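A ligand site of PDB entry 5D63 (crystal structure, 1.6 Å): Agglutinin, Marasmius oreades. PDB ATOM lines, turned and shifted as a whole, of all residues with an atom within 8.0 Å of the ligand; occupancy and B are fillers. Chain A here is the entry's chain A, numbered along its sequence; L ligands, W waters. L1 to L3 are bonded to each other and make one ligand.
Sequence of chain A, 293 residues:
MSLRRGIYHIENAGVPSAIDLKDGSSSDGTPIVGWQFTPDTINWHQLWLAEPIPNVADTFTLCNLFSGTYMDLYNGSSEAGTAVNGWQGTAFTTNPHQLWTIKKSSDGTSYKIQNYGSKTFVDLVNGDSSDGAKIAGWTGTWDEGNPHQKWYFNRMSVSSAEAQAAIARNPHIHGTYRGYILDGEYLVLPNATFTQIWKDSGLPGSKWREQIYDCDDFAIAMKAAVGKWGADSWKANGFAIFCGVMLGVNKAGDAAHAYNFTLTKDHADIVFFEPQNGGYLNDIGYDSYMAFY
OE2 of Glu 144 sits at hydrogen-bond distance from O1 of LG3 L3, 2.6 Å away.
The backbone NH of Asn 126 lies within hydrogen-bond range of an oxygen (O6) of LG2 L2 (2.8 Å).
O4 of LG2 L2 lies within hydrogen-bond range of OD2 of Asp 123.
An oxygen (O4) of LG3 L3 sits at hydrogen-bond distance from the indole nitrogen (NE1) of Trp 138.
A ring nitrogen (ND1) of His 148 sits at hydrogen-bond distance from an oxygen (O6) of LG2 L2 (3.0 Å).
The side-chain amide nitrogen (ND2) of Asn 146 sits at hydrogen-bond distance from an oxygen (O4) of LG2 L2 (2.9 Å).
O3 of LG3 L3 lies within hydrogen-bond range of OG1 of Thr 139.
NE2 of Gln 149 is in hydrogen-bond range of OD2 of Asp 123.
OD1 of Asn 146 sits at hydrogen-bond distance from N of His 148.
OE2 of Glu 144 is in salt-bridge range of NZ of Lys 112.
OE2 of Glu 144 sits at hydrogen-bond distance from N of Thr 141.
The backbone NH (N) of Val 125 sits at hydrogen-bond distance from the side-chain carboxylate (OD1) of Asp 123.
OE1 of Gln 149 lies within hydrogen-bond range of NZ of Lys 112 (2.8 Å).
The side-chain carboxylate of Glu 144 lies close to the side-chain amide oxygen of Gln 149, 3.5 Å away.
A ring nitrogen (NE2) of His 148 lies within hydrogen-bond range of the backbone NH (N) of Gly 127.
Merely in contact with the ligand: Leu 124, Val 125, Gly 140 and Gln 149.
11 residues have an atom within 4 Å of the ligand: Asp 123, Leu 124, Val 125, Asn 126, Trp 138, Thr 139, Gly 140, Glu 144, Asn 146, His 148 and Gln 149.
The nearest printed residue that does not touch the ligand is Gly 127 (4.5 Å).
Water W3 bridges O4 of LIG L1 (2.7 Å) and OD1 of Asn 146 (2.9 Å).
Water W5 lies within hydrogen-bond range of an oxygen (O5) of LG3 L3 (2.8 Å) and the indole nitrogen of Trp 138 (3.3 Å).
Water W4 lies within hydrogen-bond range of OE1 of Glu 144 (3.0 Å) and O1 of LIG L1 (3.0 Å).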
ATOM      1  N   ALA A  80      14.379 -27.651 -25.576  1.00  0.00           N
ATOM      2  CA  ALA A  80      13.809 -27.458 -24.232  1.00  0.00           C
ATOM      3  C   ALA A  80      12.344 -27.457 -24.378  1.00  0.00           C
ATOM      4  O   ALA A  80      11.803 -26.825 -25.304  1.00  0.00           O
ATOM      5  CB  ALA A  80      14.311 -26.180 -23.661  1.00  0.00           C
ATOM      6  N   GLY A  81      11.645 -28.161 -23.494  1.00  0.00           N
ATOM      7  CA  GLY A  81      10.182 -28.287 -23.583  1.00  0.00           C
ATOM      8  C   GLY A  81       9.638 -29.519 -24.261  1.00  0.00           C
ATOM      9  O   GLY A  81       8.425 -29.705 -24.346  1.00  0.00           O
ATOM     10  N   LYS A 112      19.752 -36.117 -10.789  1.00  0.00           N
ATOM     11  CA  LYS A 112      19.269 -35.614 -12.067  1.00  0.00           C
ATOM     12  C   LYS A 112      19.102 -36.762 -13.073  1.00  0.00           C
ATOM     13  O   LYS A 112      19.775 -37.821 -12.944  1.00  0.00           O
ATOM     14  CB  LYS A 112      20.142 -34.529 -12.688  1.00  0.00           C
ATOM     15  CG  LYS A 112      20.475 -33.413 -11.701  1.00  0.00           C
ATOM     16  CD  LYS A 112      21.029 -32.121 -12.314  1.00  0.00           C
ATOM     17  CE  LYS A 112      20.074 -31.511 -13.405  1.00  0.00           C
ATOM     18  NZ  LYS A 112      20.174 -30.056 -13.692  1.00  0.00           N
ATOM     19  N   PHE A 121      17.643 -32.818 -19.601  1.00  0.00           N
ATOM     20  CA  PHE A 121      17.277 -33.310 -18.313  1.00  0.00           C
ATOM     21  C   PHE A 121      15.773 -33.281 -18.122  1.00  0.00           C
ATOM     22  O   PHE A 121      15.076 -32.355 -18.601  1.00  0.00           O
ATOM     23  CB  PHE A 121      17.971 -32.449 -17.250  1.00  0.00           C
ATOM     24  CG  PHE A 121      19.463 -32.626 -17.172  1.00  0.00           C
ATOM     25  CD1 PHE A 121      19.981 -33.646 -16.418  1.00  0.00           C
ATOM     26  CD2 PHE A 121      20.304 -31.802 -17.896  1.00  0.00           C
ATOM     27  CE1 PHE A 121      21.356 -33.807 -16.343  1.00  0.00           C
ATOM     28  CE2 PHE A 121      21.712 -31.963 -17.820  1.00  0.00           C
ATOM     29  CZ  PHE A 121      22.199 -32.952 -17.049  1.00  0.00           C
ATOM     30  N   VAL A 122      15.286 -34.272 -17.376  1.00  0.00           N
ATOM     31  CA  VAL A 122      13.866 -34.274 -16.924  1.00  0.00           C
ATOM     32  C   VAL A 122      13.558 -33.118 -16.022  1.00  0.00           C
ATOM     33  O   VAL A 122      14.240 -32.840 -15.042  1.00  0.00           O
ATOM     34  CB  VAL A 122      13.545 -35.591 -16.209  1.00  0.00           C
ATOM     35  CG1 VAL A 122      12.105 -35.598 -15.711  1.00  0.00           C
ATOM     36  CG2 VAL A 122      13.772 -36.772 -17.127  1.00  0.00           C
ATOM     37  N   ASP A 123      12.561 -32.298 -16.378  1.00  0.00           N
ATOM     38  CA  ASP A 123      12.361 -30.982 -15.775  1.00  0.00           C
ATOM     39  C   ASP A 123      10.876 -30.815 -15.440  1.00  0.00           C
ATOM     40  O   ASP A 123      10.054 -30.965 -16.337  1.00  0.00           O
ATOM     41  CB  ASP A 123      12.878 -29.923 -16.786  1.00  0.00           C
ATOM     42  CG  ASP A 123      12.757 -28.486 -16.251  1.00  0.00           C
ATOM     43  OD1 ASP A 123      11.654 -28.033 -15.792  1.00  0.00           O
ATOM     44  OD2 ASP A 123      13.792 -27.726 -16.262  1.00  0.00           O
ATOM     45  N   LEU A 124      10.546 -30.531 -14.166  1.00  0.00           N
ATOM     46  CA  LEU A 124       9.179 -30.150 -13.756  1.00  0.00           C
ATOM     47  C   LEU A 124       8.997 -28.666 -14.131  1.00  0.00           C
ATOM     48  O   LEU A 124       9.557 -27.796 -13.505  1.00  0.00           O
ATOM     49  CB  LEU A 124       8.971 -30.371 -12.276  1.00  0.00           C
ATOM     50  CG  LEU A 124       7.559 -30.029 -11.814  1.00  0.00           C
ATOM     51  CD1 LEU A 124       6.466 -30.895 -12.459  1.00  0.00           C
ATOM     52  CD2 LEU A 124       7.528 -30.171 -10.318  1.00  0.00           C
ATOM     53  N   VAL A 125       8.319 -28.418 -15.250  1.00  0.00           N
ATOM     54  CA  VAL A 125       8.337 -27.089 -15.877  1.00  0.00           C
ATOM     55  C   VAL A 125       7.823 -26.005 -14.917  1.00  0.00           C
ATOM     56  O   VAL A 125       6.736 -26.116 -14.371  1.00  0.00           O
ATOM     57  CB  VAL A 125       7.627 -27.079 -17.274  1.00  0.00           C
ATOM     58  CG1 VAL A 125       7.797 -25.693 -17.924  1.00  0.00           C
ATOM     59  CG2 VAL A 125       8.197 -28.129 -18.206  1.00  0.00           C
ATOM     60  N   ASN A 126       8.674 -24.991 -14.691  1.00  0.00           N
ATOM     61  CA  ASN A 126       8.399 -23.877 -13.794  1.00  0.00           C
ATOM     62  C   ASN A 126       8.262 -24.288 -12.364  1.00  0.00           C
ATOM     63  O   ASN A 126       7.841 -23.548 -11.494  1.00  0.00           O
ATOM     64  CB  ASN A 126       7.141 -23.108 -14.189  1.00  0.00           C
ATOM     65  CG  ASN A 126       7.374 -22.197 -15.313  1.00  0.00           C
ATOM     66  OD1 ASN A 126       8.410 -21.552 -15.419  1.00  0.00           O
ATOM     67  ND2 ASN A 126       6.428 -22.140 -16.182  1.00  0.00           N
ATOM     68  N   GLY A 127       8.635 -25.507 -12.020  1.00  0.00           N
ATOM     69  CA  GLY A 127       8.455 -25.862 -10.633  1.00  0.00           C
ATOM     70  C   GLY A 127       6.989 -25.932 -10.234  1.00  0.00           C
ATOM     71  O   GLY A 127       6.625 -25.856  -9.070  1.00  0.00           O
ATOM     72  N   ASP A 128       6.147 -26.212 -11.211  1.00  0.00           N
ATOM     73  CA  ASP A 128       4.692 -26.095 -10.935  1.00  0.00           C
ATOM     74  C   ASP A 128       4.249 -27.290 -10.129  1.00  0.00           C
ATOM     75  O   ASP A 128       4.440 -28.437 -10.549  1.00  0.00           O
ATOM     76  CB  ASP A 128       3.972 -26.029 -12.289  1.00  0.00           C
ATOM     77  CG  ASP A 128       2.437 -25.945 -12.201  1.00  0.00           C
ATOM     78  OD1 ASP A 128       1.868 -25.991 -11.133  1.00  0.00           O
ATOM     79  OD2 ASP A 128       1.869 -25.786 -13.302  1.00  0.00           O
ATOM     80  N   LYS A 134       3.171 -30.163 -16.552  1.00  0.00           N
ATOM     81  CA  LYS A 134       4.062 -30.717 -17.564  1.00  0.00           C
ATOM     82  C   LYS A 134       5.488 -31.069 -17.053  1.00  0.00           C
ATOM     83  O   LYS A 134       6.108 -30.272 -16.386  1.00  0.00           O
ATOM     84  CB  LYS A 134       4.200 -29.681 -18.663  1.00  0.00           C
ATOM     85  CG  LYS A 134       5.089 -30.189 -19.852  1.00  0.00           C
ATOM     86  CD  LYS A 134       5.119 -29.232 -21.080  1.00  0.00           C
ATOM     87  CE  LYS A 134       6.121 -29.928 -21.982  1.00  0.00           C
ATOM     88  NZ  LYS A 134       5.479 -30.764 -23.039  1.00  0.00           N
ATOM     89  N   ALA A 136       9.068 -32.127 -18.930  1.00  0.00           N
ATOM     90  CA  ALA A 136       9.678 -32.038 -20.255  1.00  0.00           C
ATOM     91  C   ALA A 136      11.178 -32.302 -20.155  1.00  0.00           C
ATOM     92  O   ALA A 136      11.829 -32.183 -19.116  1.00  0.00           O
ATOM     93  CB  ALA A 136       9.483 -30.632 -20.798  1.00  0.00           C
ATOM     94  N   GLY A 137      11.760 -32.575 -21.292  1.00  0.00           N
ATOM     95  CA  GLY A 137      13.183 -32.527 -21.414  1.00  0.00           C
ATOM     96  C   GLY A 137      13.641 -31.054 -21.567  1.00  0.00           C
ATOM     97  O   GLY A 137      13.028 -30.277 -22.256  1.00  0.00           O
ATOM     98  N   TRP A 138      14.755 -30.699 -20.915  1.00  0.00           N
ATOM     99  CA  TRP A 138      15.205 -29.331 -20.887  1.00  0.00           C
ATOM    100  C   TRP A 138      16.728 -29.214 -20.786  1.00  0.00           C
ATOM    101  O   TRP A 138      17.389 -30.037 -20.139  1.00  0.00           O
ATOM    102  CB  TRP A 138      14.566 -28.642 -19.665  1.00  0.00           C
ATOM    103  CG  TRP A 138      14.334 -27.167 -19.843  1.00  0.00           C
ATOM    104  CD1 TRP A 138      15.240 -26.146 -19.800  1.00  0.00           C
ATOM    105  CD2 TRP A 138      13.049 -26.539 -20.093  1.00  0.00           C
ATOM    106  NE1 TRP A 138      14.612 -24.910 -20.006  1.00  0.00           N
ATOM    107  CE2 TRP A 138      13.259 -25.124 -20.130  1.00  0.00           C
ATOM    108  CE3 TRP A 138      11.743 -27.030 -20.224  1.00  0.00           C
ATOM    109  CZ2 TRP A 138      12.254 -24.228 -20.432  1.00  0.00           C
ATOM    110  CZ3 TRP A 138      10.732 -26.111 -20.520  1.00  0.00           C
ATOM    111  CH2 TRP A 138      11.000 -24.725 -20.585  1.00  0.00           C
ATOM    112  N   THR A 139      17.276 -28.131 -21.304  1.00  0.00           N
ATOM    113  CA  THR A 139      18.688 -27.852 -21.187  1.00  0.00           C
ATOM    114  C   THR A 139      19.017 -27.710 -19.734  1.00  0.00           C
ATOM    115  O   THR A 139      18.182 -27.288 -18.880  1.00  0.00           O
ATOM    116  CB  THR A 139      19.048 -26.527 -21.909  1.00  0.00           C
ATOM    117  OG1 THR A 139      18.174 -25.507 -21.497  1.00  0.00           O
ATOM    118  CG2 THR A 139      18.582 -26.564 -23.274  1.00  0.00           C
ATOM    119  N   GLY A 140      20.239 -28.099 -19.415  1.00  0.00           N
ATOM    120  CA  GLY A 140      20.677 -28.043 -18.020  1.00  0.00           C
ATOM    121  C   GLY A 140      22.127 -28.481 -17.855  1.00  0.00           C
ATOM    122  O   GLY A 140      22.745 -28.968 -18.838  1.00  0.00           O
ATOM    123  N   THR A 141      22.560 -28.485 -16.606  1.00  0.00           N
ATOM    124  CA  THR A 141      23.903 -28.986 -16.261  1.00  0.00           C
ATOM    125  C   THR A 141      23.837 -29.993 -15.149  1.00  0.00           C
ATOM    126  O   THR A 141      22.932 -29.999 -14.331  1.00  0.00           O
ATOM    127  CB  THR A 141      24.900 -27.864 -15.862  1.00  0.00           C
ATOM    128  OG1 THR A 141      24.527 -27.355 -14.606  1.00  0.00           O
ATOM    129  CG2 THR A 141      24.953 -26.801 -16.952  1.00  0.00           C
ATOM    130  N   GLU A 144      24.310 -27.782 -11.378  1.00  0.00           N
ATOM    131  CA  GLU A 144      23.513 -26.619 -10.931  1.00  0.00           C
ATOM    132  C   GLU A 144      22.470 -26.973  -9.891  1.00  0.00           C
ATOM    133  O   GLU A 144      22.032 -28.095  -9.779  1.00  0.00           O
ATOM    134  CB  GLU A 144      22.850 -25.922 -12.167  1.00  0.00           C
ATOM    135  CG  GLU A 144      21.896 -26.864 -12.827  1.00  0.00           C
ATOM    136  CD  GLU A 144      21.328 -26.261 -14.093  1.00  0.00           C
ATOM    137  OE1 GLU A 144      21.429 -24.998 -14.262  1.00  0.00           O
ATOM    138  OE2 GLU A 144      20.695 -27.000 -14.846  1.00  0.00           O
ATOM    139  N   GLY A 145      21.993 -25.981  -9.177  1.00  0.00           N
ATOM    140  CA  GLY A 145      21.110 -26.198  -8.113  1.00  0.00           C
ATOM    141  C   GLY A 145      19.646 -26.351  -8.468  1.00  0.00           C
ATOM    142  O   GLY A 145      18.888 -26.741  -7.628  1.00  0.00           O
ATOM    143  N   ASN A 146      19.239 -25.884  -9.658  1.00  0.00           N
ATOM    144  CA  ASN A 146      17.831 -25.738 -10.131  1.00  0.00           C
ATOM    145  C   ASN A 146      16.964 -26.916  -9.680  1.00  0.00           C
ATOM    146  O   ASN A 146      17.163 -28.043 -10.185  1.00  0.00           O
ATOM    147  CB  ASN A 146      17.909 -25.758 -11.625  1.00  0.00           C
ATOM    148  CG  ASN A 146      16.516 -25.562 -12.257  1.00  0.00           C
ATOM    149  OD1 ASN A 146      15.560 -25.466 -11.534  1.00  0.00           O
ATOM    150  ND2 ASN A 146      16.434 -25.576 -13.576  1.00  0.00           N
ATOM    151  N   PRO A 147      16.085 -26.680  -8.759  1.00  0.00           N
ATOM    152  CA  PRO A 147      15.216 -27.765  -8.232  1.00  0.00           C
ATOM    153  C   PRO A 147      14.188 -28.363  -9.203  1.00  0.00           C
ATOM    154  O   PRO A 147      13.739 -29.493  -9.018  1.00  0.00           O
ATOM    155  CB  PRO A 147      14.611 -27.161  -6.967  1.00  0.00           C
ATOM    156  CG  PRO A 147      14.638 -25.694  -7.261  1.00  0.00           C
ATOM    157  CD  PRO A 147      15.805 -25.393  -8.151  1.00  0.00           C
ATOM    158  N   HIS A 148      13.951 -27.647 -10.334  1.00  0.00           N
ATOM    159  CA  HIS A 148      13.073 -28.145 -11.398  1.00  0.00           C
ATOM    160  C   HIS A 148      13.558 -29.446 -12.024  1.00  0.00           C
ATOM    161  O   HIS A 148      12.760 -30.231 -12.523  1.00  0.00           O
ATOM    162  CB  HIS A 148      12.827 -27.133 -12.489  1.00  0.00           C
ATOM    163  CG  HIS A 148      12.299 -25.826 -12.030  1.00  0.00           C
ATOM    164  ND1 HIS A 148      12.185 -24.755 -12.873  1.00  0.00           N
ATOM    165  CD2 HIS A 148      11.918 -25.377 -10.803  1.00  0.00           C
ATOM    166  CE1 HIS A 148      11.709 -23.709 -12.228  1.00  0.00           C
ATOM    167  NE2 HIS A 148      11.580 -24.047 -10.952  1.00  0.00           N
ATOM    168  N   GLN A 149      14.874 -29.672 -11.911  1.00  0.00           N
ATOM    169  CA  GLN A 149      15.570 -30.779 -12.563  1.00  0.00           C
ATOM    170  C   GLN A 149      16.184 -31.761 -11.520  1.00  0.00           C
ATOM    171  O   GLN A 149      16.958 -32.614 -11.857  1.00  0.00           O
ATOM    172  CB  GLN A 149      16.623 -30.261 -13.498  1.00  0.00           C
ATOM    173  CG  GLN A 149      16.019 -29.459 -14.627  1.00  0.00           C
ATOM    174  CD  GLN A 149      17.043 -29.036 -15.648  1.00  0.00           C
ATOM    175  OE1 GLN A 149      18.230 -29.367 -15.530  1.00  0.00           O
ATOM    176  NE2 GLN A 149      16.593 -28.306 -16.689  1.00  0.00           N
HETATM  177  C1  LIG L   1      16.329 -21.380 -13.647  1.00  0.00           C
HETATM  178  C2  LIG L   1      17.418 -20.320 -13.797  1.00  0.00           C
HETATM  179  C3  LIG L   1      16.874 -18.941 -14.147  1.00  0.00           C
HETATM  180  C4  LIG L   1      15.909 -18.575 -13.078  1.00  0.00           C
HETATM  181  C5  LIG L   1      14.847 -19.685 -12.923  1.00  0.00           C
HETATM  182  C6  LIG L   1      13.655 -19.264 -12.054  1.00  0.00           C
HETATM  183  O1  LIG L   1      18.381 -20.603 -14.768  1.00  0.00           O
HETATM  184  O2  LIG L   1      17.898 -17.938 -14.047  1.00  0.00           O
HETATM  185  O3  LIG L   1      16.607 -18.358 -11.881  1.00  0.00           O
HETATM  186  O4  LIG L   1      15.451 -20.967 -12.615  1.00  0.00           O
HETATM  187  C1  LG2 L   2      13.325 -21.972 -15.225  1.00  0.00           C
HETATM  188  C2  LG2 L   2      14.784 -22.507 -15.079  1.00  0.00           C
HETATM  189  C3  LG2 L   2      15.193 -23.385 -16.305  1.00  0.00           C
HETATM  190  C4  LG2 L   2      14.165 -24.501 -16.512  1.00  0.00           C
HETATM  191  C5  LG2 L   2      12.771 -23.818 -16.616  1.00  0.00           C
HETATM  192  C6  LG2 L   2      11.617 -24.841 -16.827  1.00  0.00           C
HETATM  193  O1  LG2 L   2      13.413 -21.077 -16.370  1.00  0.00           O
HETATM  194  O2  LG2 L   2      15.700 -21.387 -14.925  1.00  0.00           O
HETATM  195  O3  LG2 L   2      16.555 -23.786 -16.060  1.00  0.00           O
HETATM  196  O4  LG2 L   2      14.166 -25.351 -15.327  1.00  0.00           O
HETATM  197  O5  LG2 L   2      12.445 -23.039 -15.478  1.00  0.00           O
HETATM  198  O6  LG2 L   2      11.267 -25.453 -15.617  1.00  0.00           O
HETATM  199  C1  LG3 L   3      17.112 -24.599 -17.074  1.00  0.00           C
HETATM  200  C2  LG3 L   3      18.585 -24.921 -16.817  1.00  0.00           C
HETATM  201  C3  LG3 L   3      19.359 -23.583 -16.858  1.00  0.00           C
HETATM  202  C4  LG3 L   3      19.262 -22.960 -18.237  1.00  0.00           C
HETATM  203  C5  LG3 L   3      17.705 -22.739 -18.452  1.00  0.00           C
HETATM  204  C6  LG3 L   3      17.319 -22.233 -19.854  1.00  0.00           C
HETATM  205  O1  LG3 L   3      18.641 -25.518 -15.509  1.00  0.00           O
HETATM  206  O2  LG3 L   3      20.763 -23.964 -16.674  1.00  0.00           O
HETATM  207  O3  LG3 L   3      19.668 -23.893 -19.254  1.00  0.00           O
HETATM  208  O4  LG3 L   3      16.988 -23.940 -18.275  1.00  0.00           O
HETATM  209  O5  LG3 L   3      15.852 -22.051 -20.073  1.00  0.00           O
HETATM  210  O   HOH W   1      15.644 -19.768 -17.554  1.00  0.00           O
HETATM  211  O   HOH W   2      20.135 -19.189 -15.617  1.00  0.00           O
HETATM  212  O   HOH W   3      14.857 -22.753 -10.708  1.00  0.00           O
HETATM  213  O   HOH W   4      19.238 -23.150 -13.479  1.00  0.00           O
HETATM  214  O   HOH W   5      14.692 -22.750 -22.479  1.00  0.00           O
HETATM  215  O   HOH W   6      22.525 -24.940 -19.203  1.00  0.00           O
HETATM  216  O   HOH W   7      11.553 -19.261 -15.674  1.00  0.00           O
